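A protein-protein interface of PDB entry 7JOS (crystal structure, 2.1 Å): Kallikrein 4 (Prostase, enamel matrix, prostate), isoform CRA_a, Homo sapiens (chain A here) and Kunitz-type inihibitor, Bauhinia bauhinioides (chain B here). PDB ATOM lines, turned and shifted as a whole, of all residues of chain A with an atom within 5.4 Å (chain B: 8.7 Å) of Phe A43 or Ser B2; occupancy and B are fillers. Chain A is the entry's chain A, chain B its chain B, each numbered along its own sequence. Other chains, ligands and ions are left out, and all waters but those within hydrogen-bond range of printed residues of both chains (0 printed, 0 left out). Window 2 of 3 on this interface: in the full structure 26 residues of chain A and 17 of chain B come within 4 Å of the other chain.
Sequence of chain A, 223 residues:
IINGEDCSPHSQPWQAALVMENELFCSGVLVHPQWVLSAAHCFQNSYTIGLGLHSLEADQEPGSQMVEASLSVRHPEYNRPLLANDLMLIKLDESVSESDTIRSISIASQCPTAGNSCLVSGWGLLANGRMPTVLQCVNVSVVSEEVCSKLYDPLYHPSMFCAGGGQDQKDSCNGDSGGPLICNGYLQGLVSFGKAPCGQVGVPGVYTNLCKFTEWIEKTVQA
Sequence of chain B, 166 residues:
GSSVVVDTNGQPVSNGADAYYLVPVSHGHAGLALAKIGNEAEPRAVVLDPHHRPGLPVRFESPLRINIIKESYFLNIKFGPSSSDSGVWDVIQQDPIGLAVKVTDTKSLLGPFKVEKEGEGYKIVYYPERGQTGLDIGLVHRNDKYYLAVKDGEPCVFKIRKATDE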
ATOM      1  N   ALA A  39       5.211 -10.055  11.811  1.00  0.00           N
ATOM      2  CA  ALA A  39       4.563  -9.575  13.049  1.00  0.00           C
ATOM      3  C   ALA A  39       4.368  -8.058  12.966  1.00  0.00           C
ATOM      4  O   ALA A  39       5.272  -7.366  12.485  1.00  0.00           O
ATOM      5  CB  ALA A  39       5.415  -9.977  14.230  1.00  0.00           C
ATOM      6  N   ALA A  40       3.223  -7.562  13.452  1.00  0.00           N
ATOM      7  CA  ALA A  40       2.930  -6.113  13.470  1.00  0.00           C
ATOM      8  C   ALA A  40       3.980  -5.369  14.307  1.00  0.00           C
ATOM      9  O   ALA A  40       4.293  -4.217  13.974  1.00  0.00           O
ATOM     10  CB  ALA A  40       1.534  -5.897  13.999  1.00  0.00           C
ATOM     11  N   HIS A  41       4.530  -6.018  15.331  1.00  0.00           N
ATOM     12  CA  HIS A  41       5.507  -5.309  16.193  1.00  0.00           C
ATOM     13  C   HIS A  41       6.818  -5.079  15.438  1.00  0.00           C
ATOM     14  O   HIS A  41       7.667  -4.331  15.970  1.00  0.00           O
ATOM     15  CB  HIS A  41       5.706  -6.035  17.521  1.00  0.00           C
ATOM     16  CG  HIS A  41       6.490  -7.302  17.473  1.00  0.00           C
ATOM     17  ND1 HIS A  41       5.886  -8.548  17.462  1.00  0.00           N
ATOM     18  CD2 HIS A  41       7.819  -7.523  17.482  1.00  0.00           C
ATOM     19  CE1 HIS A  41       6.820  -9.468  17.415  1.00  0.00           C
ATOM     20  NE2 HIS A  41       8.003  -8.876  17.435  1.00  0.00           N
ATOM     21  N   CYS A  42       6.969  -5.678  14.248  1.00  0.00           N
ATOM     22  CA  CYS A  42       8.194  -5.470  13.427  1.00  0.00           C
ATOM     23  C   CYS A  42       8.012  -4.274  12.493  1.00  0.00           C
ATOM     24  O   CYS A  42       8.898  -4.018  11.690  1.00  0.00           O
ATOM     25  CB  CYS A  42       8.511  -6.703  12.597  1.00  0.00           C
ATOM     26  SG  CYS A  42       8.928  -8.173  13.587  1.00  0.00           S
ATOM     27  N   PHE A  43       6.890  -3.570  12.598  1.00  0.00           N
ATOM     28  CA  PHE A  43       6.597  -2.442  11.681  1.00  0.00           C
ATOM     29  C   PHE A  43       7.777  -1.460  11.580  1.00  0.00           C
ATOM     30  O   PHE A  43       8.398  -1.164  12.592  1.00  0.00           O
ATOM     31  CB  PHE A  43       5.373  -1.680  12.166  1.00  0.00           C
ATOM     32  CG  PHE A  43       5.100  -0.444  11.351  1.00  0.00           C
ATOM     33  CD1 PHE A  43       4.352  -0.515  10.190  1.00  0.00           C
ATOM     34  CD2 PHE A  43       5.611   0.788  11.744  1.00  0.00           C
ATOM     35  CE1 PHE A  43       4.118   0.615   9.428  1.00  0.00           C
ATOM     36  CE2 PHE A  43       5.365   1.923  10.987  1.00  0.00           C
ATOM     37  CZ  PHE A  43       4.623   1.836   9.832  1.00  0.00           C
ATOM     38  N   GLN A  44       8.040  -0.976  10.371  1.00  0.00           N
ATOM     39  CA  GLN A  44       8.986   0.141  10.068  1.00  0.00           C
ATOM     40  C   GLN A  44       8.388   0.945   8.905  1.00  0.00           C
ATOM     41  O   GLN A  44       7.526   0.383   8.168  1.00  0.00           O
ATOM     42  CB  GLN A  44      10.373  -0.375   9.687  1.00  0.00           C
ATOM     43  CG  GLN A  44      11.144  -0.981  10.839  1.00  0.00           C
ATOM     44  CD  GLN A  44      11.599   0.066  11.831  1.00  0.00           C
ATOM     45  OE1 GLN A  44      12.615   0.729  11.639  1.00  0.00           O
ATOM     46  NE2 GLN A  44      10.844   0.229  12.904  1.00  0.00           N
ATOM     47  N   ASN A  45       8.797   2.203   8.750  1.00  0.00           N
ATOM     48  CA  ASN A  45       8.256   3.076   7.667  1.00  0.00           C
ATOM     49  C   ASN A  45       8.748   2.574   6.315  1.00  0.00           C
ATOM     50  O   ASN A  45       8.063   2.800   5.306  1.00  0.00           O
ATOM     51  CB  ASN A  45       8.603   4.548   7.912  1.00  0.00           C
ATOM     52  CG  ASN A  45       7.898   5.052   9.150  1.00  0.00           C
ATOM     53  OD1 ASN A  45       6.680   5.054   9.203  1.00  0.00           O
ATOM     54  ND2 ASN A  45       8.648   5.405  10.168  1.00  0.00           N
ATOM     55  N   TYR A  47      11.358  -0.857   4.342  1.00  0.00           N
ATOM     56  CA  TYR A  47      12.075  -2.120   4.647  1.00  0.00           C
ATOM     57  C   TYR A  47      13.023  -2.435   3.494  1.00  0.00           C
ATOM     58  O   TYR A  47      12.725  -2.121   2.312  1.00  0.00           O
ATOM     59  CB  TYR A  47      11.089  -3.294   4.788  1.00  0.00           C
ATOM     60  CG  TYR A  47       9.919  -3.084   5.721  1.00  0.00           C
ATOM     61  CD1 TYR A  47       8.729  -2.530   5.269  1.00  0.00           C
ATOM     62  CD2 TYR A  47       9.971  -3.501   7.037  1.00  0.00           C
ATOM     63  CE1 TYR A  47       7.637  -2.369   6.104  1.00  0.00           C
ATOM     64  CE2 TYR A  47       8.887  -3.340   7.899  1.00  0.00           C
ATOM     65  CZ  TYR A  47       7.722  -2.771   7.432  1.00  0.00           C
ATOM     66  OH  TYR A  47       6.644  -2.599   8.258  1.00  0.00           O
ATOM     67  N   SER A  72       3.245  -0.869   4.592  1.00  0.00           N
ATOM     68  CA  SER A  72       2.775  -2.013   5.397  1.00  0.00           C
ATOM     69  C   SER A  72       1.375  -1.750   5.952  1.00  0.00           C
ATOM     70  O   SER A  72       0.987  -0.597   6.097  1.00  0.00           O
ATOM     71  CB  SER A  72       3.740  -2.453   6.438  1.00  0.00           C
ATOM     72  OG  SER A  72       4.509  -1.430   6.975  1.00  0.00           O
ATOM     73  N   ARG A  74      -0.744  -3.020   9.173  1.00  0.00           N
ATOM     74  CA  ARG A  74      -0.899  -3.758  10.455  1.00  0.00           C
ATOM     75  C   ARG A  74      -2.354  -4.177  10.612  1.00  0.00           C
ATOM     76  O   ARG A  74      -3.242  -3.453  10.160  1.00  0.00           O
ATOM     77  CB  ARG A  74      -0.438  -2.909  11.625  1.00  0.00           C
ATOM     78  CG  ARG A  74       1.029  -2.515  11.525  1.00  0.00           C
ATOM     79  CD  ARG A  74       1.527  -1.776  12.730  1.00  0.00           C
ATOM     80  NE  ARG A  74       0.580  -0.811  13.226  1.00  0.00           N
ATOM     81  CZ  ARG A  74       0.724  -0.119  14.340  1.00  0.00           C
ATOM     82  NH1 ARG A  74       1.836  -0.226  15.051  1.00  0.00           N
ATOM     83  NH2 ARG A  74      -0.259   0.682  14.739  1.00  0.00           N
ATOM     84  N   MET A  88       1.081  -8.296  10.227  1.00  0.00           N
ATOM     85  CA  MET A  88       1.021  -7.178   9.258  1.00  0.00           C
ATOM     86  C   MET A  88       1.455  -7.681   7.878  1.00  0.00           C
ATOM     87  O   MET A  88       2.207  -8.662   7.797  1.00  0.00           O
ATOM     88  CB  MET A  88       1.876  -5.981   9.701  1.00  0.00           C
ATOM     89  CG  MET A  88       3.330  -6.190   9.611  1.00  0.00           C
ATOM     90  SD  MET A  88       4.276  -4.635   9.775  1.00  0.00           S
ATOM     91  CE  MET A  88       5.884  -5.421   9.733  1.00  0.00           C
ATOM     92  N   SER B   2       6.672   2.099  15.390  1.00  0.00           N
ATOM     93  CA  SER B   2       7.601   2.730  14.376  1.00  0.00           C
ATOM     94  C   SER B   2       8.936   3.195  14.995  1.00  0.00           C
ATOM     95  O   SER B   2       9.994   3.009  14.296  1.00  0.00           O
ATOM     96  CB  SER B   2       6.927   3.871  13.630  1.00  0.00           C
ATOM     97  OG  SER B   2       6.095   4.650  14.481  1.00  0.00           O
ATOM     98  N   SER B   3       8.923   3.760  16.221  1.00  0.00           N
ATOM     99  CA  SER B   3      10.039   4.648  16.686  1.00  0.00           C
ATOM    100  C   SER B   3      11.092   3.896  17.513  1.00  0.00           C
ATOM    101  O   SER B   3      10.828   3.583  18.688  1.00  0.00           O
ATOM    102  CB  SER B   3       9.507   5.814  17.437  1.00  0.00           C
ATOM    103  OG  SER B   3       9.772   6.982  16.679  1.00  0.00           O
ATOM    104  N   VAL B   4      12.259   3.646  16.920  1.00  0.00           N
ATOM    105  CA  VAL B   4      13.302   2.797  17.556  1.00  0.00           C
ATOM    106  C   VAL B   4      14.057   3.653  18.579  1.00  0.00           C
ATOM    107  O   VAL B   4      14.399   4.796  18.257  1.00  0.00           O
ATOM    108  CB  VAL B   4      14.237   2.202  16.506  1.00  0.00           C
ATOM    109  CG1 VAL B   4      15.405   1.462  17.129  1.00  0.00           C
ATOM    110  CG2 VAL B   4      13.479   1.279  15.562  1.00  0.00           C
ATOM    111  N   VAL B   5      14.255   3.123  19.785  1.00  0.00           N
ATOM    112  CA  VAL B   5      15.045   3.824  20.835  1.00  0.00           C
ATOM    113  C   VAL B   5      16.520   3.654  20.490  1.00  0.00           C
ATOM    114  O   VAL B   5      16.940   2.498  20.248  1.00  0.00           O
ATOM    115  CB  VAL B   5      14.711   3.248  22.218  1.00  0.00           C
ATOM    116  CG1 VAL B   5      15.531   3.894  23.314  1.00  0.00           C
ATOM    117  CG2 VAL B   5      13.236   3.410  22.528  1.00  0.00           C
ATOM    118  N   ILE B  66      11.821  -9.752  19.200  1.00  0.00           N
ATOM    119  CA  ILE B  66      12.640  -8.812  18.375  1.00  0.00           C
ATOM    120  C   ILE B  66      13.881  -8.434  19.207  1.00  0.00           C
ATOM    121  O   ILE B  66      13.856  -8.587  20.444  1.00  0.00           O
ATOM    122  CB  ILE B  66      11.755  -7.615  17.993  1.00  0.00           C
ATOM    123  CG1 ILE B  66      12.436  -6.741  16.939  1.00  0.00           C
ATOM    124  CG2 ILE B  66      11.299  -6.850  19.242  1.00  0.00           C
ATOM    125  CD1 ILE B  66      11.493  -5.712  16.335  1.00  0.00           C
ATOM    126  N   ILE B  68      15.439  -5.444  19.205  1.00  0.00           N
ATOM    127  CA  ILE B  68      15.538  -3.979  19.452  1.00  0.00           C
ATOM    128  C   ILE B  68      14.292  -3.537  20.211  1.00  0.00           C
ATOM    129  O   ILE B  68      13.327  -4.306  20.269  1.00  0.00           O
ATOM    130  CB  ILE B  68      15.652  -3.191  18.133  1.00  0.00           C
ATOM    131  CG1 ILE B  68      14.371  -3.343  17.302  1.00  0.00           C
ATOM    132  CG2 ILE B  68      16.900  -3.605  17.363  1.00  0.00           C
ATOM    133  CD1 ILE B  68      14.356  -2.501  16.071  1.00  0.00           C
ATOM    134  N   ILE B  69      14.313  -2.285  20.656  1.00  0.00           N
ATOM    135  CA  ILE B  69      13.278  -1.671  21.526  1.00  0.00           C
ATOM    136  C   ILE B  69      12.706  -0.475  20.780  1.00  0.00           C
ATOM    137  O   ILE B  69      13.477   0.330  20.253  1.00  0.00           O
ATOM    138  CB  ILE B  69      13.894  -1.263  22.880  1.00  0.00           C
ATOM    139  CG1 ILE B  69      14.286  -2.486  23.688  1.00  0.00           C
ATOM    140  CG2 ILE B  69      13.006  -0.358  23.675  1.00  0.00           C
ATOM    141  CD1 ILE B  69      13.198  -3.468  23.842  1.00  0.00           C
ATOM    142  N   LYS B  70      11.383  -0.355  20.792  1.00  0.00           N
ATOM    143  CA  LYS B  70      10.694   0.839  20.271  1.00  0.00           C
ATOM    144  C   LYS B  70       9.991   1.567  21.411  1.00  0.00           C
ATOM    145  O   LYS B  70       9.681   0.942  22.446  1.00  0.00           O
ATOM    146  CB  LYS B  70       9.629   0.418  19.254  1.00  0.00           C
ATOM    147  CG  LYS B  70      10.105  -0.270  17.976  1.00  0.00           C
ATOM    148  CD  LYS B  70       8.949  -0.403  17.022  1.00  0.00           C
ATOM    149  CE  LYS B  70       9.181  -1.293  15.826  1.00  0.00           C
ATOM    150  NZ  LYS B  70       7.893  -1.533  15.119  1.00  0.00           N
ATOM    151  N   GLU B  71       9.682   2.835  21.188  1.00  0.00           N
ATOM    152  CA  GLU B  71       9.022   3.690  22.196  1.00  0.00           C
ATOM    153  C   GLU B  71       7.602   3.197  22.475  1.00  0.00           C
ATOM    154  O   GLU B  71       7.046   3.607  23.523  1.00  0.00           O
ATOM    155  CB  GLU B  71       8.934   5.130  21.690  1.00  0.00           C
ATOM    156  CG  GLU B  71      10.284   5.747  21.398  1.00  0.00           C
ATOM    157  CD  GLU B  71      10.245   7.208  20.965  1.00  0.00           C
ATOM    158  OE1 GLU B  71       9.333   7.958  21.422  1.00  0.00           O
ATOM    159  OE2 GLU B  71      11.125   7.588  20.157  1.00  0.00           O
ATOM    160  N   SER B  72       7.035   2.377  21.587  1.00  0.00           N
ATOM    161  CA  SER B  72       5.624   1.947  21.791  1.00  0.00           C
ATOM    162  C   SER B  72       5.570   0.675  22.646  1.00  0.00           C
ATOM    163  O   SER B  72       4.471   0.359  23.108  1.00  0.00           O
ATOM    164  CB  SER B  72       4.944   1.732  20.465  1.00  0.00           C
ATOM    165  OG  SER B  72       5.645   0.757  19.709  1.00  0.00           O
ATOM    166  N   TYR B  73       6.718   0.013  22.868  1.00  0.00           N
ATOM    167  CA  TYR B  73       6.740  -1.259  23.638  1.00  0.00           C
ATOM    168  C   TYR B  73       6.624  -1.026  25.148  1.00  0.00           C
ATOM    169  O   TYR B  73       7.297  -0.135  25.726  1.00  0.00           O
ATOM    170  CB  TYR B  73       8.033  -2.027  23.414  1.00  0.00           C
ATOM    171  CG  TYR B  73       8.301  -2.515  22.006  1.00  0.00           C
ATOM    172  CD1 TYR B  73       7.339  -2.492  21.009  1.00  0.00           C
ATOM    173  CD2 TYR B  73       9.514  -3.084  21.700  1.00  0.00           C
ATOM    174  CE1 TYR B  73       7.596  -2.975  19.735  1.00  0.00           C
ATOM    175  CE2 TYR B  73       9.784  -3.580  20.433  1.00  0.00           C
ATOM    176  CZ  TYR B  73       8.831  -3.513  19.445  1.00  0.00           C
ATOM    177  OH  TYR B  73       9.162  -4.000  18.211  1.00  0.00           O
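The side-chain amide nitrogen (NE2) of Gln A44 is in hydrogen-bond range of the backbone carbonyl oxygen (O) of Ser B2 (3.2 Å). The backbone carbonyl oxygen of His A41 sits at hydrogen-bond distance from the side-chain hydroxyl of Tyr B73 (2.7 Å). NZ of Lys B70 lies within hydrogen-bond range of O of Phe A43, at 2.6 Å. The side-chain amino group (NZ) of Lys B70 sits at hydrogen-bond distance from the backbone carbonyl oxygen (O) of His A41 (2.9 Å).
The side-chain hydroxyl (OH) of Tyr A47 is in hydrogen-bond range of the backbone NH (N) of Gln A44 (3.0 Å).
Among the printed residues, merely in contact across the chains: His A41 with Ile B66, Cys A42 with Lys B70, Phe A43 with Ser B2, Gln A44 with Val B4 and Gln A44 with Lys B70.
Of the printed residues of chain B, His A41 touches Ile B66 (3.96 Å), Lys B70 (2.9 Å) and Tyr B73 (2.7 Å). Phe A43 touches two residues of chain B. Printed residues of chain B within 4 Å of Gln A44: Ser B2 (3.2 Å), Val B4 (3.9 Å) and Lys B70 (3.7 Å). Ser B2 touches just these residues of chain A: Phe A43 and Gln A44. Printed residues of chain A within 4 Å of Ile B66: His A41. Glu B71 touches none of the printed residues of chain A. Ser B72 touches none of the printed residues of chain A. Printed residues of chain A within 4 Å of Tyr B73: His A41. The nearest residue of chain B that does not touch Phe A43 is Tyr B73 (6.1 Å).
Of the 11 printed residues of chain A, 4 touch a printed residue of chain B. Printed residues of chain A that touch a printed residue of chain B: His A41, Cys A42, Phe A43 and Gln A44. Hydrophobic or aromatic side chains of chain A within 4 Å of the printed part of chain B: His A41 and Phe A43.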
